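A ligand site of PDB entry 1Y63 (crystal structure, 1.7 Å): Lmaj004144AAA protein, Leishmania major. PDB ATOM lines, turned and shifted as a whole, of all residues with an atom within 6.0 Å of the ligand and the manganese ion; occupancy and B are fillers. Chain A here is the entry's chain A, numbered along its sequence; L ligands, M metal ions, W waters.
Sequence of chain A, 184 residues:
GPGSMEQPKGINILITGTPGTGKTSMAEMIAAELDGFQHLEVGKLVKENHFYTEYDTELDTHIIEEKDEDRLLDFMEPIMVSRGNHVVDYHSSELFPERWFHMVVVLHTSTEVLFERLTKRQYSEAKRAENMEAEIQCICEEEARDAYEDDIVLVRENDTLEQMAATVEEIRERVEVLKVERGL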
ATOM      1  N   GLY A  17      20.490  -7.923   9.234  1.00  0.00           N
ATOM      2  CA  GLY A  17      19.608  -8.916   9.816  1.00  0.00           C
ATOM      3  C   GLY A  17      18.168  -8.464   9.722  1.00  0.00           C
ATOM      4  O   GLY A  17      17.877  -7.275   9.604  1.00  0.00           O
ATOM      5  N   THR A  18      17.273  -9.427   9.774  1.00  0.00           N
ATOM      6  CA  THR A  18      15.847  -9.168   9.794  1.00  0.00           C
ATOM      7  C   THR A  18      15.457  -8.154  10.882  1.00  0.00           C
ATOM      8  O   THR A  18      16.067  -8.119  11.979  1.00  0.00           O
ATOM      9  CB  THR A  18      15.109 -10.480  10.096  1.00  0.00           C
ATOM     10  OG1 THR A  18      15.581 -11.488   9.227  1.00  0.00           O
ATOM     11  CG2 THR A  18      13.633 -10.331   9.952  1.00  0.00           C
ATOM     12  N   PRO A  19      14.459  -7.294  10.585  1.00  0.00           N
ATOM     13  CA  PRO A  19      13.898  -6.488  11.667  1.00  0.00           C
ATOM     14  C   PRO A  19      13.589  -7.337  12.911  1.00  0.00           C
ATOM     15  O   PRO A  19      13.007  -8.426  12.813  1.00  0.00           O
ATOM     16  CB  PRO A  19      12.621  -5.923  11.040  1.00  0.00           C
ATOM     17  CG  PRO A  19      12.973  -5.794   9.594  1.00  0.00           C
ATOM     18  CD  PRO A  19      13.775  -7.015   9.300  1.00  0.00           C
ATOM     19  N   GLY A  20      14.031  -6.835  14.052  1.00  0.00           N
ATOM     20  CA  GLY A  20      13.820  -7.445  15.349  1.00  0.00           C
ATOM     21  C   GLY A  20      14.979  -8.335  15.830  1.00  0.00           C
ATOM     22  O   GLY A  20      14.930  -8.805  16.973  1.00  0.00           O
ATOM     23  N   THR A  21      15.988  -8.580  14.988  1.00  0.00           N
ATOM     24  CA  THR A  21      17.129  -9.415  15.384  1.00  0.00           C
ATOM     25  C   THR A  21      18.130  -8.796  16.358  1.00  0.00           C
ATOM     26  O   THR A  21      18.975  -9.501  16.931  1.00  0.00           O
ATOM     27  CB  THR A  21      17.900  -9.962  14.143  1.00  0.00           C
ATOM     28  OG1 THR A  21      18.281  -8.873  13.283  1.00  0.00           O
ATOM     29  CG2 THR A  21      17.014 -10.951  13.404  1.00  0.00           C
ATOM     30  N   GLY A  22      18.082  -7.475  16.503  1.00  0.00           N
ATOM     31  CA  GLY A  22      18.906  -6.771  17.475  1.00  0.00           C
ATOM     32  C   GLY A  22      19.945  -5.824  16.934  1.00  0.00           C
ATOM     33  O   GLY A  22      20.907  -5.515  17.647  1.00  0.00           O
ATOM     34  N   LYS A  23      19.777  -5.375  15.693  1.00  0.00           N
ATOM     35  CA  LYS A  23      20.810  -4.557  15.013  1.00  0.00           C
ATOM     36  C   LYS A  23      21.105  -3.261  15.735  1.00  0.00           C
ATOM     37  O   LYS A  23      22.249  -2.928  16.030  1.00  0.00           O
ATOM     38  CB  LYS A  23      20.417  -4.257  13.571  1.00  0.00           C
ATOM     39  CG  LYS A  23      20.160  -5.454  12.696  1.00  0.00           C
ATOM     40  CD  LYS A  23      19.712  -5.030  11.316  1.00  0.00           C
ATOM     41  CE  LYS A  23      18.391  -4.323  11.293  1.00  0.00           C
ATOM     42  NZ  LYS A  23      17.280  -5.244  11.731  1.00  0.00           N
ATOM     43  N   THR A  24      20.047  -2.505  16.037  1.00  0.00           N
ATOM     44  CA  THR A  24      20.208  -1.211  16.681  1.00  0.00           C
ATOM     45  C   THR A  24      20.771  -1.367  18.075  1.00  0.00           C
ATOM     46  O   THR A  24      21.687  -0.603  18.480  1.00  0.00           O
ATOM     47  CB  THR A  24      18.877  -0.439  16.664  1.00  0.00           C
ATOM     48  OG1 THR A  24      18.455  -0.245  15.311  1.00  0.00           O
ATOM     49  CG2 THR A  24      19.046   0.927  17.377  1.00  0.00           C
ATOM     50  N   SER A  25      20.285  -2.364  18.800  1.00  0.00           N
ATOM     51  CA  SER A  25      20.801  -2.648  20.141  1.00  0.00           C
ATOM     52  C   SER A  25      22.289  -2.971  20.123  1.00  0.00           C
ATOM     53  O   SER A  25      23.062  -2.497  20.947  1.00  0.00           O
ATOM     54  CB  SER A  25      20.014  -3.770  20.795  1.00  0.00           C
ATOM     55  OG  SER A  25      18.659  -3.394  20.939  1.00  0.00           O
ATOM     56  N   MET A  26      22.686  -3.829  19.184  1.00  0.00           N
ATOM     57  CA  MET A  26      24.103  -4.194  19.064  1.00  0.00           C
ATOM     58  C   MET A  26      24.949  -3.013  18.611  1.00  0.00           C
ATOM     59  O   MET A  26      26.017  -2.788  19.148  1.00  0.00           O
ATOM     60  CB  MET A  26      24.325  -5.371  18.133  1.00  0.00           C
ATOM     61  CG  MET A  26      25.774  -5.818  18.130  1.00  0.00           C
ATOM     62  SD  MET A  26      26.047  -7.291  17.136  1.00  0.00           S
ATOM     63  CE  MET A  26      25.294  -8.520  18.200  1.00  0.00           C
ATOM     64  N   GLU A  41      22.105   4.925  11.960  1.00  0.00           N
ATOM     65  CA  GLU A  41      20.873   4.161  11.905  1.00  0.00           C
ATOM     66  C   GLU A  41      20.215   4.476  10.561  1.00  0.00           C
ATOM     67  O   GLU A  41      19.509   5.443  10.425  1.00  0.00           O
ATOM     68  CB  GLU A  41      19.967   4.519  13.123  1.00  0.00           C
ATOM     69  CG  GLU A  41      18.787   3.606  13.365  1.00  0.00           C
ATOM     70  CD  GLU A  41      18.151   3.728  14.761  1.00  0.00           C
ATOM     71  OE1 GLU A  41      18.741   4.316  15.709  1.00  0.00           O
ATOM     72  OE2 GLU A  41      17.007   3.262  14.909  1.00  0.00           O
ATOM     73  N   ASP A  89      23.848   0.398  10.605  1.00  0.00           N
ATOM     74  CA  ASP A  89      22.785  -0.462  11.096  1.00  0.00           C
ATOM     75  C   ASP A  89      21.654  -0.437  10.072  1.00  0.00           C
ATOM     76  O   ASP A  89      21.053   0.612   9.883  1.00  0.00           O
ATOM     77  CB  ASP A  89      22.393   0.144  12.454  1.00  0.00           C
ATOM     78  CG  ASP A  89      21.034  -0.188  12.923  1.00  0.00           C
ATOM     79  OD1 ASP A  89      20.386  -1.083  12.408  1.00  0.00           O
ATOM     80  OD2 ASP A  89      20.658   0.458  13.945  1.00  0.00           O
ATOM     81  N   LEU A 107      22.866 -10.846  12.029  1.00  0.00           N
ATOM     82  CA  LEU A 107      22.224 -11.342  13.217  1.00  0.00           C
ATOM     83  C   LEU A 107      21.051 -12.246  12.878  1.00  0.00           C
ATOM     84  O   LEU A 107      20.284 -11.964  11.968  1.00  0.00           O
ATOM     85  CB  LEU A 107      21.735 -10.188  14.102  1.00  0.00           C
ATOM     86  CG  LEU A 107      22.788  -9.136  14.486  1.00  0.00           C
ATOM     87  CD1 LEU A 107      22.197  -8.056  15.380  1.00  0.00           C
ATOM     88  CD2 LEU A 107      23.937  -9.819  15.123  1.00  0.00           C
ATOM     89  N   ARG A 117       9.737 -10.211  20.260  1.00  0.00           N
ATOM     90  CA  ARG A 117      10.308  -8.889  20.056  1.00  0.00           C
ATOM     91  C   ARG A 117       9.447  -8.039  19.130  1.00  0.00           C
ATOM     92  O   ARG A 117       9.244  -6.858  19.349  1.00  0.00           O
ATOM     93  CB  ARG A 117      11.702  -9.013  19.469  1.00  0.00           C
ATOM     94  CG  ARG A 117      12.713  -9.555  20.419  1.00  0.00           C
ATOM     95  CD  ARG A 117      14.061  -9.634  19.756  1.00  0.00           C
ATOM     96  NE  ARG A 117      15.067 -10.270  20.634  1.00  0.00           N
ATOM     97  CZ  ARG A 117      16.315 -10.522  20.249  1.00  0.00           C
ATOM     98  NH1 ARG A 117      16.733 -10.202  19.016  1.00  0.00           N
ATOM     99  NH2 ARG A 117      17.143 -11.154  21.057  1.00  0.00           N
ATOM    100  N   ARG A 121       7.533  -4.726  20.221  1.00  0.00           N
ATOM    101  CA  ARG A 121       7.833  -3.531  19.473  1.00  0.00           C
ATOM    102  C   ARG A 121       6.658  -3.070  18.582  1.00  0.00           C
ATOM    103  O   ARG A 121       6.798  -2.151  17.784  1.00  0.00           O
ATOM    104  CB  ARG A 121       9.126  -3.731  18.654  1.00  0.00           C
ATOM    105  CG  ARG A 121      10.388  -4.009  19.508  1.00  0.00           C
ATOM    106  CD  ARG A 121      10.851  -2.796  20.314  1.00  0.00           C
ATOM    107  NE  ARG A 121      11.617  -1.850  19.503  1.00  0.00           N
ATOM    108  CZ  ARG A 121      11.872  -0.595  19.851  1.00  0.00           C
ATOM    109  NH1 ARG A 121      11.422  -0.096  20.996  1.00  0.00           N
ATOM    110  NH2 ARG A 121      12.588   0.186  19.046  1.00  0.00           N
ATOM    111  N   TYR A 123       4.838  -4.186  15.869  1.00  0.00           N
ATOM    112  CA  TYR A 123       4.659  -4.291  14.413  1.00  0.00           C
ATOM    113  C   TYR A 123       3.209  -4.769  14.162  1.00  0.00           C
ATOM    114  O   TYR A 123       2.652  -5.455  15.017  1.00  0.00           O
ATOM    115  CB  TYR A 123       5.653  -5.287  13.811  1.00  0.00           C
ATOM    116  CG  TYR A 123       7.102  -4.838  13.811  1.00  0.00           C
ATOM    117  CD1 TYR A 123       7.811  -4.630  14.998  1.00  0.00           C
ATOM    118  CD2 TYR A 123       7.790  -4.661  12.600  1.00  0.00           C
ATOM    119  CE1 TYR A 123       9.151  -4.244  14.979  1.00  0.00           C
ATOM    120  CE2 TYR A 123       9.131  -4.261  12.586  1.00  0.00           C
ATOM    121  CZ  TYR A 123       9.803  -4.058  13.770  1.00  0.00           C
ATOM    122  OH  TYR A 123      11.122  -3.673  13.737  1.00  0.00           O
ATOM    123  N   ASN A 158      21.634 -14.251  18.011  1.00  0.00           N
ATOM    124  CA  ASN A 158      21.489 -13.076  18.875  1.00  0.00           C
ATOM    125  C   ASN A 158      20.177 -13.109  19.633  1.00  0.00           C
ATOM    126  O   ASN A 158      19.368 -12.210  19.490  1.00  0.00           O
ATOM    127  CB  ASN A 158      21.594 -11.786  18.040  1.00  0.00           C
ATOM    128  CG  ASN A 158      21.926 -10.576  18.866  1.00  0.00           C
ATOM    129  OD1 ASN A 158      22.852 -10.625  19.699  1.00  0.00           O
ATOM    130  ND2 ASN A 158      21.194  -9.461  18.662  1.00  0.00           N
ATOM    131  N   ASP A 159      19.985 -14.167  20.422  1.00  0.00           N
ATOM    132  CA  ASP A 159      18.738 -14.373  21.192  1.00  0.00           C
ATOM    133  C   ASP A 159      18.790 -13.710  22.580  1.00  0.00           C
ATOM    134  O   ASP A 159      17.749 -13.247  23.102  1.00  0.00           O
ATOM    135  CB  ASP A 159      18.477 -15.867  21.414  1.00  0.00           C
ATOM    136  CG  ASP A 159      18.000 -16.587  20.174  1.00  0.00           C
ATOM    137  OD1 ASP A 159      17.550 -15.946  19.206  1.00  0.00           O
ATOM    138  OD2 ASP A 159      18.003 -17.829  20.186  1.00  0.00           O
ATOM    139  N   THR A 160      19.986 -13.701  23.158  1.00  0.00           N
ATOM    140  CA  THR A 160      20.221 -13.235  24.545  1.00  0.00           C
ATOM    141  C   THR A 160      21.274 -12.125  24.668  1.00  0.00           C
ATOM    142  O   THR A 160      22.066 -11.892  23.762  1.00  0.00           O
ATOM    143  CB  THR A 160      20.714 -14.411  25.423  1.00  0.00           C
ATOM    144  OG1 THR A 160      22.050 -14.776  25.067  1.00  0.00           O
ATOM    145  CG2 THR A 160      19.800 -15.613  25.264  1.00  0.00           C
ATOM    146  N   LEU A 161      21.275 -11.452  25.812  1.00  0.00           N
ATOM    147  CA  LEU A 161      22.215 -10.378  26.067  1.00  0.00           C
ATOM    148  C   LEU A 161      23.631 -10.916  26.172  1.00  0.00           C
ATOM    149  O   LEU A 161      24.596 -10.285  25.723  1.00  0.00           O
ATOM    150  CB  LEU A 161      21.803  -9.627  27.342  1.00  0.00           C
ATOM    151  CG  LEU A 161      22.621  -8.375  27.665  1.00  0.00           C
ATOM    152  CD1 LEU A 161      22.613  -7.325  26.530  1.00  0.00           C
ATOM    153  CD2 LEU A 161      22.083  -7.766  28.909  1.00  0.00           C
ATOM    154  N   GLU A 162      23.761 -12.106  26.747  1.00  0.00           N
ATOM    155  CA  GLU A 162      25.046 -12.803  26.810  1.00  0.00           C
ATOM    156  C   GLU A 162      25.604 -13.026  25.412  1.00  0.00           C
ATOM    157  O   GLU A 162      26.796 -12.828  25.185  1.00  0.00           O
ATOM    158  CB  GLU A 162      24.923 -14.125  27.571  1.00  0.00           C
ATOM    159  CG  GLU A 162      26.132 -15.030  27.513  1.00  0.00           C
ATOM    160  CD  GLU A 162      25.892 -16.330  28.249  1.00  0.00           C
ATOM    161  OE1 GLU A 162      25.560 -16.263  29.446  1.00  0.00           O
ATOM    162  OE2 GLU A 162      26.028 -17.404  27.624  1.00  0.00           O
ATOM    163  N   GLN A 163      24.748 -13.453  24.493  1.00  0.00           N
ATOM    164  CA  GLN A 163      25.158 -13.606  23.111  1.00  0.00           C
ATOM    165  C   GLN A 163      25.587 -12.288  22.503  1.00  0.00           C
ATOM    166  O   GLN A 163      26.635 -12.219  21.868  1.00  0.00           O
ATOM    167  CB  GLN A 163      24.082 -14.261  22.287  1.00  0.00           C
ATOM    168  CG  GLN A 163      24.010 -15.745  22.578  1.00  0.00           C
ATOM    169  CD  GLN A 163      22.895 -16.421  21.838  1.00  0.00           C
ATOM    170  OE1 GLN A 163      21.882 -15.789  21.525  1.00  0.00           O
ATOM    171  NE2 GLN A 163      23.077 -17.707  21.537  1.00  0.00           N
ATOM    172  N   MET A 164      24.805 -11.237  22.704  1.00  0.00           N
ATOM    173  CA  MET A 164      25.172  -9.925  22.184  1.00  0.00           C
ATOM    174  C   MET A 164      26.532  -9.494  22.674  1.00  0.00           C
ATOM    175  O   MET A 164      27.343  -9.032  21.884  1.00  0.00           O
ATOM    176  CB  MET A 164      24.104  -8.865  22.561  1.00  0.00           C
ATOM    177  CG  MET A 164      24.320  -7.545  21.813  1.00  0.00           C
ATOM    178  SD  MET A 164      22.787  -6.686  21.362  1.00  0.00           S
ATOM    179  CE  MET A 164      22.219  -6.314  23.011  1.00  0.00           C
HETATM  180  P1  LIG L   1      16.426  -4.254  15.143  1.00  0.00           P
HETATM  181  O1  LIG L   1      15.030  -4.176  14.563  1.00  0.00           O
HETATM  182  O2  LIG L   1      17.201  -5.384  14.482  1.00  0.00           O
HETATM  183  O3  LIG L   1      17.176  -2.924  15.180  1.00  0.00           O
HETATM  184  P2  LIG L   1      16.423  -3.943  18.031  1.00  0.00           P
HETATM  185  O4  LIG L   1      17.876  -3.639  18.365  1.00  0.00           O
HETATM  186  O5  LIG L   1      15.495  -2.734  17.943  1.00  0.00           O
HETATM  187  O6  LIG L   1      16.303  -4.787  16.692  1.00  0.00           O
HETATM  188  O7  LIG L   1      15.831  -4.986  19.081  1.00  0.00           O
HETATM  189  C1  LIG L   1      14.460  -4.890  19.455  1.00  0.00           C
HETATM  190  C2  LIG L   1      14.397  -5.307  20.906  1.00  0.00           C
HETATM  191  O8  LIG L   1      14.910  -6.635  21.045  1.00  0.00           O
HETATM  192  C3  LIG L   1      15.266  -4.463  21.837  1.00  0.00           C
HETATM  193  O9  LIG L   1      14.644  -3.239  22.222  1.00  0.00           O
HETATM  194  C4  LIG L   1      15.467  -5.407  22.984  1.00  0.00           C
HETATM  195  O10 LIG L   1      14.296  -5.483  23.779  1.00  0.00           O
HETATM  196  C5  LIG L   1      15.587  -6.736  22.297  1.00  0.00           C
HETATM  197  N1  LIG L   1      16.941  -7.231  22.004  1.00  0.00           N
HETATM  198  C6  LIG L   1      17.790  -6.915  20.970  1.00  0.00           C
HETATM  199  N2  LIG L   1      18.914  -7.650  21.015  1.00  0.00           N
HETATM  200  C7  LIG L   1      18.777  -8.494  22.099  1.00  0.00           C
HETATM  201  C8  LIG L   1      19.614  -9.523  22.694  1.00  0.00           C
HETATM  202  N3  LIG L   1      20.806  -9.841  22.148  1.00  0.00           N
HETATM  203  N4  LIG L   1      19.125 -10.148  23.782  1.00  0.00           N
HETATM  204  C9  LIG L   1      17.905  -9.814  24.308  1.00  0.00           C
HETATM  205  N5  LIG L   1      17.067  -8.881  23.831  1.00  0.00           N
HETATM  206  C10 LIG L   1      17.486  -8.201  22.725  1.00  0.00           C
HETATM  207 MN    MN M   1      16.658  -1.013  14.460  1.00  0.00          MN
HETATM  208  O   HOH W   1      15.573  -0.585  16.333  1.00  0.00           O
HETATM  209  O   HOH W   2      14.450 -11.051  23.353  1.00  0.00           O
HETATM  210  O   HOH W   3      12.605  -3.933  15.846  1.00  0.00           O
HETATM  211  O   HOH W   4      15.061  -1.513  20.324  1.00  0.00           O
HETATM  212  O   HOH W   5      14.809  -1.842  13.494  1.00  0.00           O
HETATM  213  O   HOH W   6      17.785  -1.255  12.650  1.00  0.00           O
HETATM  214  O   HOH W   7      16.038   1.000  13.763  1.00  0.00           O
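N of Thr 24 is in hydrogen-bond range of O4 of the ligand, 3.4 Å away.
The backbone NH of Ser 25 lies within hydrogen-bond range of an oxygen (O4) of the ligand (2.8 Å).
The side-chain hydroxyl (OG) of Ser 25 lies within hydrogen-bond range of an oxygen (O4) of the ligand (2.7 Å).
O2 of the ligand lies within hydrogen-bond range of N of Lys 23.
The side-chain amino group (NZ) of Lys 23 is in salt-bridge range of an oxygen (O2) of the ligand (2.8 Å).
O1 of the ligand lies within hydrogen-bond range of N of Gly 20, 2.9 Å away.
N3 of the ligand is in hydrogen-bond range of O of Thr 160 (2.9 Å).
The backbone NH (N) of Gly 22 sits at hydrogen-bond distance from an oxygen (O2) of the ligand.
N of Leu 161 sits at hydrogen-bond distance from N4 of the ligand (3.2 Å).
OD1 of Asn 158 lies within hydrogen-bond range of N3 of the ligand (3.3 Å).
The backbone NH (N) of Thr 21 lies within hydrogen-bond range of an oxygen (O2) of the ligand, at 3.5 Å.
The side-chain amino group (NZ) of Lys 23 sits at hydrogen-bond distance from the backbone carbonyl oxygen (O) of Thr 18, at 3.1 Å.
The backbone carbonyl oxygen of Gly 17 lies within hydrogen-bond range of the side-chain amino group of Lys 23.
O of Gly 20 sits close to NH1 of Arg 117 (3.1 Å).
The backbone NH (N) of Gln 163 sits at hydrogen-bond distance from the side-chain hydroxyl (OG1) of Thr 160 (3.1 Å).
The guanidinium group (NH1) of Arg 117 sits at hydrogen-bond distance from the backbone carbonyl oxygen (O) of Thr 21, at 3.1 Å.
OG1 of Thr 21 sits at hydrogen-bond distance from O of Thr 18 (2.7 Å).
N of Asp 159 is in hydrogen-bond range of OE1 of Gln 163, at 2.7 Å.
The side-chain sulfur (SD) of Met 164 sits at hydrogen-bond distance from the backbone NH (N) of Met 26, at 3.6 Å.
O of Asp 159 sits close to N4 of the ligand (3.5 Å).
Residues that only touch the ligand: Thr 18, Pro 19, Arg 117 and Met 164.
Hydrophobic or aromatic side chains that line the ligand: Met 164.
14 residues have an atom within 4 Å of the ligand: Thr 18, Pro 19, Gly 20, Thr 21, Gly 22, Lys 23, Thr 24, Ser 25, Arg 117, Asn 158, Asp 159, Thr 160, Leu 161 and Met 164.
The manganese ion is bound by O3 of the ligand (2.1 Å), OG1 of Thr 24 (2.1 Å), water W6 (2.1 Å), water W1 (2.2 Å), water W7 (2.2 Å) and water W5 (2.2 Å).
The manganese ion has six donor atoms within binding distance.
Water W4 lies within hydrogen-bond range of an oxygen (O9) of the ligand (2.6 Å) and the guanidinium group (NH2) of Arg 121 (3.3 Å).
Water W3 bridges OH of Tyr 123 (2.6 Å) and O1 of the ligand (2.8 Å).
Water W2 bridges the guanidinium group of Arg 117 (2.9 Å) and a nitrogen (N5) of the ligand (3.4 Å).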
